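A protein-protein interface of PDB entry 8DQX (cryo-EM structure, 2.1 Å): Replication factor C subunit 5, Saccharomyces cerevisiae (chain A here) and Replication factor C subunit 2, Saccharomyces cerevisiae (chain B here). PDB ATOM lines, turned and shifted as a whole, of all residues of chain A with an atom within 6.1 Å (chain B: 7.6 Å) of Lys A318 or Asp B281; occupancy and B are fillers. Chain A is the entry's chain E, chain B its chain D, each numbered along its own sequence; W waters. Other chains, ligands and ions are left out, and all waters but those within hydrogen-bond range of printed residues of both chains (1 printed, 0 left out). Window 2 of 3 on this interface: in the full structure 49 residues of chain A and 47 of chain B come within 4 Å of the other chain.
OD2 of Asp B281 is in salt-bridge range of NZ of Lys A318, at 3.9 Å. The side-chain amide nitrogen (ND2) of Asn B345 lies within hydrogen-bond range of the side-chain carboxylate (OE1) of Glu A323, 3.3 Å away. The side-chain amide nitrogen (NE2) of Gln B352 sits at hydrogen-bond distance from the side-chain hydroxyl (OG) of Ser A319, at 2.8 Å.
The side-chain carboxylate (OD1) of Asp B279 sits at hydrogen-bond distance from the backbone NH (N) of Asp B281 (2.9 Å). The side-chain carboxylate of Asp B281 is in salt-bridge range of the side-chain amino group of Lys B284 (3.2 Å). The backbone carbonyl oxygen (O) of Thr A315 sits at hydrogen-bond distance from the side-chain hydroxyl (OG) of Ser A319 (2.8 Å).
Phe B280 touches Leu A308 (CZ to CD2, 3.7 Å). O of Leu A308 touches CE of Lys B284 (3.8 Å). Thr A315 touches Gln B352. Phe B280 touches Lys A318. CE2 of Phe B280 touches N of Ser A319, at 3.9 Å. OG of Ser A319 touches CG1 of Val B348, 3.8 Å away. Ile A322 touches Asn B345 (CG1 to N, 3.8 Å).
Printed residues of chain B within 4 Å of Leu A308: Phe B280 and Lys B284. Val A310 touches none of the printed residues of chain B. Lys A318 touches two residues of chain B. Asp B281 touches just one residue of chain A: Lys A318 (3.9 Å). Glu B282 touches none of the printed residues of chain A. Of the printed residues of chain A, Lys B284 touches Leu A308 (3.8 Å). Of the printed residues of chain A, Asn B345 touches Ile A322 (3.8 Å) and Glu A323 (3.3 Å). Printed residues of chain A within 4 Å of Val B348: Ser A319 (3.8 Å). The nearest residue of chain B that does not touch Lys A318 is Lys B284 (5.8 Å). The nearest residue of chain A that does not touch Asp B281 is Leu A308 (4.5 Å).
Hydrophobic or aromatic side chains of chain B within 4 Å of the printed part of chain A: Phe B280 and Val B348. Among the printed residues, 10 pairs touch across the chains.
Water W1 bridges the side-chain amide oxygen of Asn B345 (2.9 Å) and the backbone carbonyl oxygen of Ser A319 (3.1 Å).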
ATOM      1  N   LEU A 307       2.039  -8.988  18.956  1.00  0.00           N
ATOM      2  CA  LEU A 307       3.073  -9.964  19.276  1.00  0.00           C
ATOM      3  C   LEU A 307       2.562 -11.385  19.086  1.00  0.00           C
ATOM      4  O   LEU A 307       3.248 -12.229  18.499  1.00  0.00           O
ATOM      5  CB  LEU A 307       3.556  -9.762  20.711  1.00  0.00           C
ATOM      6  CG  LEU A 307       4.499  -8.581  20.939  1.00  0.00           C
ATOM      7  CD1 LEU A 307       4.497  -8.168  22.401  1.00  0.00           C
ATOM      8  CD2 LEU A 307       5.902  -8.932  20.473  1.00  0.00           C
ATOM      9  N   LEU A 308       1.352 -11.667  19.573  1.00  0.00           N
ATOM     10  CA  LEU A 308       0.825 -13.022  19.469  1.00  0.00           C
ATOM     11  C   LEU A 308       0.593 -13.445  18.022  1.00  0.00           C
ATOM     12  O   LEU A 308       0.440 -14.641  17.759  1.00  0.00           O
ATOM     13  CB  LEU A 308      -0.474 -13.145  20.268  1.00  0.00           C
ATOM     14  CG  LEU A 308      -0.347 -12.976  21.785  1.00  0.00           C
ATOM     15  CD1 LEU A 308      -1.727 -12.952  22.428  1.00  0.00           C
ATOM     16  CD2 LEU A 308       0.512 -14.067  22.398  1.00  0.00           C
ATOM     17  N   ASP A 309       0.560 -12.500  17.084  1.00  0.00           N
ATOM     18  CA  ASP A 309       0.413 -12.830  15.672  1.00  0.00           C
ATOM     19  C   ASP A 309       1.736 -13.152  14.988  1.00  0.00           C
ATOM     20  O   ASP A 309       1.719 -13.636  13.852  1.00  0.00           O
ATOM     21  CB  ASP A 309      -0.260 -11.676  14.930  1.00  0.00           C
ATOM     22  CG  ASP A 309      -1.758 -11.637  15.147  1.00  0.00           C
ATOM     23  OD1 ASP A 309      -2.361 -12.712  15.332  1.00  0.00           O
ATOM     24  OD2 ASP A 309      -2.334 -10.529  15.129  1.00  0.00           O
ATOM     25  N   VAL A 310       2.874 -12.898  15.639  1.00  0.00           N
ATOM     26  CA  VAL A 310       4.163 -13.127  14.995  1.00  0.00           C
ATOM     27  C   VAL A 310       4.323 -14.608  14.689  1.00  0.00           C
ATOM     28  O   VAL A 310       4.185 -15.466  15.570  1.00  0.00           O
ATOM     29  CB  VAL A 310       5.305 -12.603  15.879  1.00  0.00           C
ATOM     30  CG1 VAL A 310       6.662 -12.974  15.277  1.00  0.00           C
ATOM     31  CG2 VAL A 310       5.194 -11.099  16.049  1.00  0.00           C
ATOM     32  N   GLU A 311       4.635 -14.916  13.430  1.00  0.00           N
ATOM     33  CA  GLU A 311       4.659 -16.307  12.990  1.00  0.00           C
ATOM     34  C   GLU A 311       5.851 -17.072  13.557  1.00  0.00           C
ATOM     35  O   GLU A 311       5.771 -18.291  13.732  1.00  0.00           O
ATOM     36  CB  GLU A 311       4.669 -16.362  11.463  1.00  0.00           C
ATOM     37  CG  GLU A 311       3.573 -15.534  10.806  1.00  0.00           C
ATOM     38  CD  GLU A 311       4.001 -14.104  10.526  1.00  0.00           C
ATOM     39  OE1 GLU A 311       4.583 -13.466  11.432  1.00  0.00           O
ATOM     40  OE2 GLU A 311       3.754 -13.616   9.403  1.00  0.00           O
ATOM     41  N   LEU A 313       7.244 -17.103  16.534  1.00  0.00           N
ATOM     42  CA  LEU A 313       7.262 -17.456  17.947  1.00  0.00           C
ATOM     43  C   LEU A 313       6.598 -18.809  18.189  1.00  0.00           C
ATOM     44  O   LEU A 313       5.725 -19.244  17.435  1.00  0.00           O
ATOM     45  CB  LEU A 313       6.565 -16.373  18.773  1.00  0.00           C
ATOM     46  CG  LEU A 313       7.133 -14.962  18.569  1.00  0.00           C
ATOM     47  CD1 LEU A 313       6.449 -13.958  19.476  1.00  0.00           C
ATOM     48  CD2 LEU A 313       8.639 -14.949  18.803  1.00  0.00           C
ATOM     49  N   ASN A 314       7.025 -19.476  19.262  1.00  0.00           N
ATOM     50  CA  ASN A 314       6.501 -20.778  19.639  1.00  0.00           C
ATOM     51  C   ASN A 314       5.474 -20.627  20.762  1.00  0.00           C
ATOM     52  O   ASN A 314       5.234 -19.535  21.284  1.00  0.00           O
ATOM     53  CB  ASN A 314       7.638 -21.720  20.052  1.00  0.00           C
ATOM     54  CG  ASN A 314       8.433 -21.201  21.236  1.00  0.00           C
ATOM     55  OD1 ASN A 314       7.886 -20.956  22.309  1.00  0.00           O
ATOM     56  ND2 ASN A 314       9.735 -21.043  21.048  1.00  0.00           N
ATOM     57  N   THR A 315       4.868 -21.753  21.145  1.00  0.00           N
ATOM     58  CA  THR A 315       3.796 -21.720  22.136  1.00  0.00           C
ATOM     59  C   THR A 315       4.290 -21.185  23.476  1.00  0.00           C
ATOM     60  O   THR A 315       3.581 -20.427  24.150  1.00  0.00           O
ATOM     61  CB  THR A 315       3.191 -23.118  22.295  1.00  0.00           C
ATOM     62  OG1 THR A 315       2.407 -23.433  21.138  1.00  0.00           O
ATOM     63  CG2 THR A 315       2.303 -23.192  23.526  1.00  0.00           C
ATOM     64  N   THR A 316       5.507 -21.560  23.876  1.00  0.00           N
ATOM     65  CA  THR A 316       6.046 -21.106  25.157  1.00  0.00           C
ATOM     66  C   THR A 316       6.167 -19.585  25.195  1.00  0.00           C
ATOM     67  O   THR A 316       5.737 -18.936  26.162  1.00  0.00           O
ATOM     68  CB  THR A 316       7.406 -21.767  25.405  1.00  0.00           C
ATOM     69  OG1 THR A 316       7.278 -23.187  25.281  1.00  0.00           O
ATOM     70  CG2 THR A 316       7.928 -21.433  26.788  1.00  0.00           C
ATOM     71  N   ASN A 317       6.737 -18.997  24.139  1.00  0.00           N
ATOM     72  CA  ASN A 317       6.851 -17.544  24.067  1.00  0.00           C
ATOM     73  C   ASN A 317       5.482 -16.888  24.192  1.00  0.00           C
ATOM     74  O   ASN A 317       5.301 -15.934  24.958  1.00  0.00           O
ATOM     75  CB  ASN A 317       7.509 -17.117  22.750  1.00  0.00           C
ATOM     76  CG  ASN A 317       8.880 -17.738  22.531  1.00  0.00           C
ATOM     77  OD1 ASN A 317       9.248 -18.040  21.396  1.00  0.00           O
ATOM     78  ND2 ASN A 317       9.643 -17.911  23.598  1.00  0.00           N
ATOM     79  N   LYS A 318       4.502 -17.392  23.442  1.00  0.00           N
ATOM     80  CA  LYS A 318       3.186 -16.763  23.408  1.00  0.00           C
ATOM     81  C   LYS A 318       2.490 -16.847  24.763  1.00  0.00           C
ATOM     82  O   LYS A 318       1.852 -15.878  25.200  1.00  0.00           O
ATOM     83  CB  LYS A 318       2.335 -17.415  22.319  1.00  0.00           C
ATOM     84  CG  LYS A 318       2.257 -16.611  21.032  1.00  0.00           C
ATOM     85  CD  LYS A 318       2.743 -17.392  19.834  1.00  0.00           C
ATOM     86  CE  LYS A 318       1.957 -18.680  19.648  1.00  0.00           C
ATOM     87  NZ  LYS A 318       2.015 -19.179  18.256  1.00  0.00           N
ATOM     88  N   SER A 319       2.592 -17.996  25.436  1.00  0.00           N
ATOM     89  CA  SER A 319       1.996 -18.129  26.762  1.00  0.00           C
ATOM     90  C   SER A 319       2.647 -17.170  27.752  1.00  0.00           C
ATOM     91  O   SER A 319       1.958 -16.529  28.561  1.00  0.00           O
ATOM     92  CB  SER A 319       2.114 -19.572  27.251  1.00  0.00           C
ATOM     93  OG  SER A 319       1.692 -20.480  26.254  1.00  0.00           O
ATOM     94  N   SER A 320       3.976 -17.039  27.690  1.00  0.00           N
ATOM     95  CA  SER A 320       4.640 -16.051  28.533  1.00  0.00           C
ATOM     96  C   SER A 320       4.115 -14.651  28.241  1.00  0.00           C
ATOM     97  O   SER A 320       3.861 -13.867  29.165  1.00  0.00           O
ATOM     98  CB  SER A 320       6.154 -16.105  28.321  1.00  0.00           C
ATOM     99  OG  SER A 320       6.681 -17.357  28.703  1.00  0.00           O
ATOM    100  N   ILE A 321       3.948 -14.321  26.958  1.00  0.00           N
ATOM    101  CA  ILE A 321       3.533 -12.971  26.591  1.00  0.00           C
ATOM    102  C   ILE A 321       2.143 -12.671  27.141  1.00  0.00           C
ATOM    103  O   ILE A 321       1.899 -11.586  27.678  1.00  0.00           O
ATOM    104  CB  ILE A 321       3.599 -12.782  25.063  1.00  0.00           C
ATOM    105  CG1 ILE A 321       5.058 -12.734  24.602  1.00  0.00           C
ATOM    106  CG2 ILE A 321       2.871 -11.510  24.640  1.00  0.00           C
ATOM    107  CD1 ILE A 321       5.237 -12.871  23.095  1.00  0.00           C
ATOM    108  N   ILE A 322       1.212 -13.623  27.021  1.00  0.00           N
ATOM    109  CA  ILE A 322      -0.151 -13.357  27.482  1.00  0.00           C
ATOM    110  C   ILE A 322      -0.202 -13.279  29.012  1.00  0.00           C
ATOM    111  O   ILE A 322      -0.941 -12.458  29.574  1.00  0.00           O
ATOM    112  CB  ILE A 322      -1.143 -14.392  26.910  1.00  0.00           C
ATOM    113  CG1 ILE A 322      -2.594 -13.977  27.199  1.00  0.00           C
ATOM    114  CG2 ILE A 322      -0.884 -15.785  27.471  1.00  0.00           C
ATOM    115  CD1 ILE A 322      -3.021 -12.666  26.560  1.00  0.00           C
ATOM    116  N   GLU A 323       0.589 -14.103  29.713  1.00  0.00           N
ATOM    117  CA  GLU A 323       0.693 -13.943  31.168  1.00  0.00           C
ATOM    118  C   GLU A 323       1.194 -12.553  31.555  1.00  0.00           C
ATOM    119  O   GLU A 323       0.618 -11.892  32.433  1.00  0.00           O
ATOM    120  CB  GLU A 323       1.608 -15.014  31.762  1.00  0.00           C
ATOM    121  CG  GLU A 323       1.756 -14.912  33.284  1.00  0.00           C
ATOM    122  CD  GLU A 323       0.481 -15.152  34.066  1.00  0.00           C
ATOM    123  OE1 GLU A 323      -0.437 -14.303  34.014  1.00  0.00           O
ATOM    124  OE2 GLU A 323       0.427 -16.162  34.797  1.00  0.00           O
ATOM    125  N   CYS A 352      11.781 -12.966  27.864  1.00  0.00           N
ATOM    126  CA  CYS A 352      11.208 -14.274  27.559  1.00  0.00           C
ATOM    127  C   CYS A 352      11.574 -14.776  26.164  1.00  0.00           C
ATOM    128  O   CYS A 352      11.567 -15.989  25.944  1.00  0.00           O
ATOM    129  CB  CYS A 352       9.688 -14.226  27.713  1.00  0.00           C
ATOM    130  SG  CYS A 352       8.767 -14.163  26.167  1.00  0.00           S
ATOM    131  N   LYS B 274     -12.223 -26.407  22.709  1.00  0.00           N
ATOM    132  CA  LYS B 274     -11.016 -25.704  22.283  1.00  0.00           C
ATOM    133  C   LYS B 274      -9.926 -25.801  23.344  1.00  0.00           C
ATOM    134  O   LYS B 274      -8.744 -25.973  23.022  1.00  0.00           O
ATOM    135  CB  LYS B 274     -11.330 -24.239  21.975  1.00  0.00           C
ATOM    136  CG  LYS B 274     -12.062 -24.023  20.665  1.00  0.00           C
ATOM    137  CD  LYS B 274     -11.159 -24.278  19.470  1.00  0.00           C
ATOM    138  CE  LYS B 274     -11.955 -24.397  18.188  1.00  0.00           C
ATOM    139  NZ  LYS B 274     -12.855 -23.239  17.991  1.00  0.00           N
ATOM    140  N   GLY B 278      -6.015 -27.696  23.051  1.00  0.00           N
ATOM    141  CA  GLY B 278      -4.773 -27.139  23.544  1.00  0.00           C
ATOM    142  C   GLY B 278      -3.940 -26.356  22.548  1.00  0.00           C
ATOM    143  O   GLY B 278      -2.835 -25.932  22.901  1.00  0.00           O
ATOM    144  N   ASP B 279      -4.425 -26.138  21.328  1.00  0.00           N
ATOM    145  CA  ASP B 279      -3.670 -25.390  20.327  1.00  0.00           C
ATOM    146  C   ASP B 279      -3.800 -23.892  20.594  1.00  0.00           C
ATOM    147  O   ASP B 279      -4.904 -23.343  20.541  1.00  0.00           O
ATOM    148  CB  ASP B 279      -4.173 -25.738  18.927  1.00  0.00           C
ATOM    149  CG  ASP B 279      -3.359 -25.085  17.834  1.00  0.00           C
ATOM    150  OD1 ASP B 279      -3.184 -23.851  17.866  1.00  0.00           O
ATOM    151  OD2 ASP B 279      -2.893 -25.812  16.932  1.00  0.00           O
ATOM    152  N   PHE B 280      -2.670 -23.231  20.857  1.00  0.00           N
ATOM    153  CA  PHE B 280      -2.708 -21.825  21.254  1.00  0.00           C
ATOM    154  C   PHE B 280      -3.410 -20.974  20.206  1.00  0.00           C
ATOM    155  O   PHE B 280      -4.283 -20.165  20.532  1.00  0.00           O
ATOM    156  CB  PHE B 280      -1.290 -21.299  21.499  1.00  0.00           C
ATOM    157  CG  PHE B 280      -1.254 -19.897  22.067  1.00  0.00           C
ATOM    158  CD1 PHE B 280      -1.472 -18.794  21.254  1.00  0.00           C
ATOM    159  CD2 PHE B 280      -1.015 -19.685  23.414  1.00  0.00           C
ATOM    160  CE1 PHE B 280      -1.451 -17.506  21.777  1.00  0.00           C
ATOM    161  CE2 PHE B 280      -0.987 -18.404  23.941  1.00  0.00           C
ATOM    162  CZ  PHE B 280      -1.207 -17.314  23.120  1.00  0.00           C
ATOM    163  N   ASP B 281      -3.035 -21.135  18.937  1.00  0.00           N
ATOM    164  CA  ASP B 281      -3.589 -20.281  17.894  1.00  0.00           C
ATOM    165  C   ASP B 281      -5.093 -20.481  17.755  1.00  0.00           C
ATOM    166  O   ASP B 281      -5.840 -19.512  17.566  1.00  0.00           O
ATOM    167  CB  ASP B 281      -2.881 -20.554  16.569  1.00  0.00           C
ATOM    168  CG  ASP B 281      -1.705 -19.626  16.335  1.00  0.00           C
ATOM    169  OD1 ASP B 281      -0.879 -19.924  15.445  1.00  0.00           O
ATOM    170  OD2 ASP B 281      -1.599 -18.601  17.039  1.00  0.00           O
ATOM    171  N   GLU B 282      -5.556 -21.730  17.836  1.00  0.00           N
ATOM    172  CA  GLU B 282      -6.987 -21.991  17.736  1.00  0.00           C
ATOM    173  C   GLU B 282      -7.743 -21.336  18.884  1.00  0.00           C
ATOM    174  O   GLU B 282      -8.791 -20.712  18.672  1.00  0.00           O
ATOM    175  CB  GLU B 282      -7.245 -23.500  17.724  1.00  0.00           C
ATOM    176  CG  GLU B 282      -6.881 -24.229  16.428  1.00  0.00           C
ATOM    177  CD  GLU B 282      -6.976 -23.366  15.181  1.00  0.00           C
ATOM    178  OE1 GLU B 282      -7.963 -22.613  15.041  1.00  0.00           O
ATOM    179  OE2 GLU B 282      -6.057 -23.439  14.337  1.00  0.00           O
ATOM    180  N   ILE B 283      -7.229 -21.468  20.108  1.00  0.00           N
ATOM    181  CA  ILE B 283      -7.870 -20.823  21.249  1.00  0.00           C
ATOM    182  C   ILE B 283      -7.901 -19.314  21.046  1.00  0.00           C
ATOM    183  O   ILE B 283      -8.917 -18.661  21.301  1.00  0.00           O
ATOM    184  CB  ILE B 283      -7.152 -21.201  22.559  1.00  0.00           C
ATOM    185  CG1 ILE B 283      -7.240 -22.713  22.804  1.00  0.00           C
ATOM    186  CG2 ILE B 283      -7.744 -20.421  23.736  1.00  0.00           C
ATOM    187  CD1 ILE B 283      -6.338 -23.215  23.899  1.00  0.00           C
ATOM    188  N   LYS B 284      -6.788 -18.740  20.590  1.00  0.00           N
ATOM    189  CA  LYS B 284      -6.719 -17.297  20.380  1.00  0.00           C
ATOM    190  C   LYS B 284      -7.778 -16.834  19.384  1.00  0.00           C
ATOM    191  O   LYS B 284      -8.511 -15.870  19.639  1.00  0.00           O
ATOM    192  CB  LYS B 284      -5.320 -16.916  19.890  1.00  0.00           C
ATOM    193  CG  LYS B 284      -5.156 -15.449  19.541  1.00  0.00           C
ATOM    194  CD  LYS B 284      -3.711 -15.071  19.227  1.00  0.00           C
ATOM    195  CE  LYS B 284      -3.024 -16.064  18.292  1.00  0.00           C
ATOM    196  NZ  LYS B 284      -3.768 -16.261  17.025  1.00  0.00           N
ATOM    197  N   LYS B 285      -7.868 -17.510  18.237  1.00  0.00           N
ATOM    198  CA  LYS B 285      -8.832 -17.105  17.218  1.00  0.00           C
ATOM    199  C   LYS B 285     -10.262 -17.269  17.716  1.00  0.00           C
ATOM    200  O   LYS B 285     -11.118 -16.397  17.489  1.00  0.00           O
ATOM    201  CB  LYS B 285      -8.612 -17.913  15.941  1.00  0.00           C
ATOM    202  CG  LYS B 285      -7.393 -17.474  15.154  1.00  0.00           C
ATOM    203  CD  LYS B 285      -6.746 -18.632  14.401  1.00  0.00           C
ATOM    204  CE  LYS B 285      -7.380 -18.842  13.034  1.00  0.00           C
ATOM    205  NZ  LYS B 285      -8.867 -18.895  13.081  1.00  0.00           N
ATOM    206  N   TYR B 286     -10.543 -18.376  18.408  1.00  0.00           N
ATOM    207  CA  TYR B 286     -11.889 -18.572  18.925  1.00  0.00           C
ATOM    208  C   TYR B 286     -12.244 -17.493  19.939  1.00  0.00           C
ATOM    209  O   TYR B 286     -13.365 -16.979  19.930  1.00  0.00           O
ATOM    210  CB  TYR B 286     -12.043 -19.958  19.550  1.00  0.00           C
ATOM    211  CG  TYR B 286     -13.480 -20.240  19.925  1.00  0.00           C
ATOM    212  CD1 TYR B 286     -14.364 -20.795  19.007  1.00  0.00           C
ATOM    213  CD2 TYR B 286     -13.965 -19.914  21.185  1.00  0.00           C
ATOM    214  CE1 TYR B 286     -15.681 -21.039  19.344  1.00  0.00           C
ATOM    215  CE2 TYR B 286     -15.277 -20.146  21.530  1.00  0.00           C
ATOM    216  CZ  TYR B 286     -16.134 -20.706  20.605  1.00  0.00           C
ATOM    217  OH  TYR B 286     -17.440 -20.943  20.947  1.00  0.00           O
ATOM    218  N   VAL B 287     -11.306 -17.136  20.818  1.00  0.00           N
ATOM    219  CA  VAL B 287     -11.580 -16.111  21.822  1.00  0.00           C
ATOM    220  C   VAL B 287     -11.821 -14.765  21.154  1.00  0.00           C
ATOM    221  O   VAL B 287     -12.698 -13.997  21.569  1.00  0.00           O
ATOM    222  CB  VAL B 287     -10.427 -16.039  22.842  1.00  0.00           C
ATOM    223  CG1 VAL B 287     -10.560 -14.794  23.722  1.00  0.00           C
ATOM    224  CG2 VAL B 287     -10.399 -17.290  23.684  1.00  0.00           C
ATOM    225  N   LEU B 344      -8.306 -14.739  27.720  1.00  0.00           N
ATOM    226  CA  LEU B 344      -7.382 -15.537  26.920  1.00  0.00           C
ATOM    227  C   LEU B 344      -6.297 -16.156  27.793  1.00  0.00           C
ATOM    228  O   LEU B 344      -5.943 -17.330  27.622  1.00  0.00           O
ATOM    229  CB  LEU B 344      -6.759 -14.689  25.812  1.00  0.00           C
ATOM    230  CG  LEU B 344      -5.780 -15.450  24.908  1.00  0.00           C
ATOM    231  CD1 LEU B 344      -6.412 -16.736  24.383  1.00  0.00           C
ATOM    232  CD2 LEU B 344      -5.304 -14.575  23.766  1.00  0.00           C
ATOM    233  N   ASN B 345      -5.754 -15.381  28.736  1.00  0.00           N
ATOM    234  CA  ASN B 345      -4.750 -15.925  29.640  1.00  0.00           C
ATOM    235  C   ASN B 345      -5.306 -17.114  30.415  1.00  0.00           C
ATOM    236  O   ASN B 345      -4.658 -18.166  30.514  1.00  0.00           O
ATOM    237  CB  ASN B 345      -4.261 -14.838  30.597  1.00  0.00           C
ATOM    238  CG  ASN B 345      -3.219 -15.347  31.572  1.00  0.00           C
ATOM    239  OD1 ASN B 345      -2.238 -15.970  31.175  1.00  0.00           O
ATOM    240  ND2 ASN B 345      -3.434 -15.095  32.853  1.00  0.00           N
ATOM    241  N   VAL B 348      -5.672 -20.238  28.089  1.00  0.00           N
ATOM    242  CA  VAL B 348      -4.378 -20.840  27.775  1.00  0.00           C
ATOM    243  C   VAL B 348      -3.865 -21.637  28.971  1.00  0.00           C
ATOM    244  O   VAL B 348      -3.426 -22.794  28.836  1.00  0.00           O
ATOM    245  CB  VAL B 348      -3.382 -19.745  27.341  1.00  0.00           C
ATOM    246  CG1 VAL B 348      -1.958 -20.293  27.262  1.00  0.00           C
ATOM    247  CG2 VAL B 348      -3.805 -19.143  26.008  1.00  0.00           C
ATOM    248  N   GLN B 352      -3.071 -25.816  29.293  1.00  0.00           N
ATOM    249  CA  GLN B 352      -1.780 -26.429  29.582  1.00  0.00           C
ATOM    250  C   GLN B 352      -1.765 -27.229  30.886  1.00  0.00           C
ATOM    251  O   GLN B 352      -0.690 -27.642  31.330  1.00  0.00           O
ATOM    252  CB  GLN B 352      -0.688 -25.359  29.588  1.00  0.00           C
ATOM    253  CG  GLN B 352      -0.453 -24.790  28.189  1.00  0.00           C
ATOM    254  CD  GLN B 352       0.292 -23.473  28.181  1.00  0.00           C
ATOM    255  OE1 GLN B 352       0.653 -22.937  29.227  1.00  0.00           O
ATOM    256  NE2 GLN B 352       0.521 -22.938  26.985  1.00  0.00           N
HETATM  257  O   HOH W   1      -0.569 -17.912  29.725  1.00  0.00           O
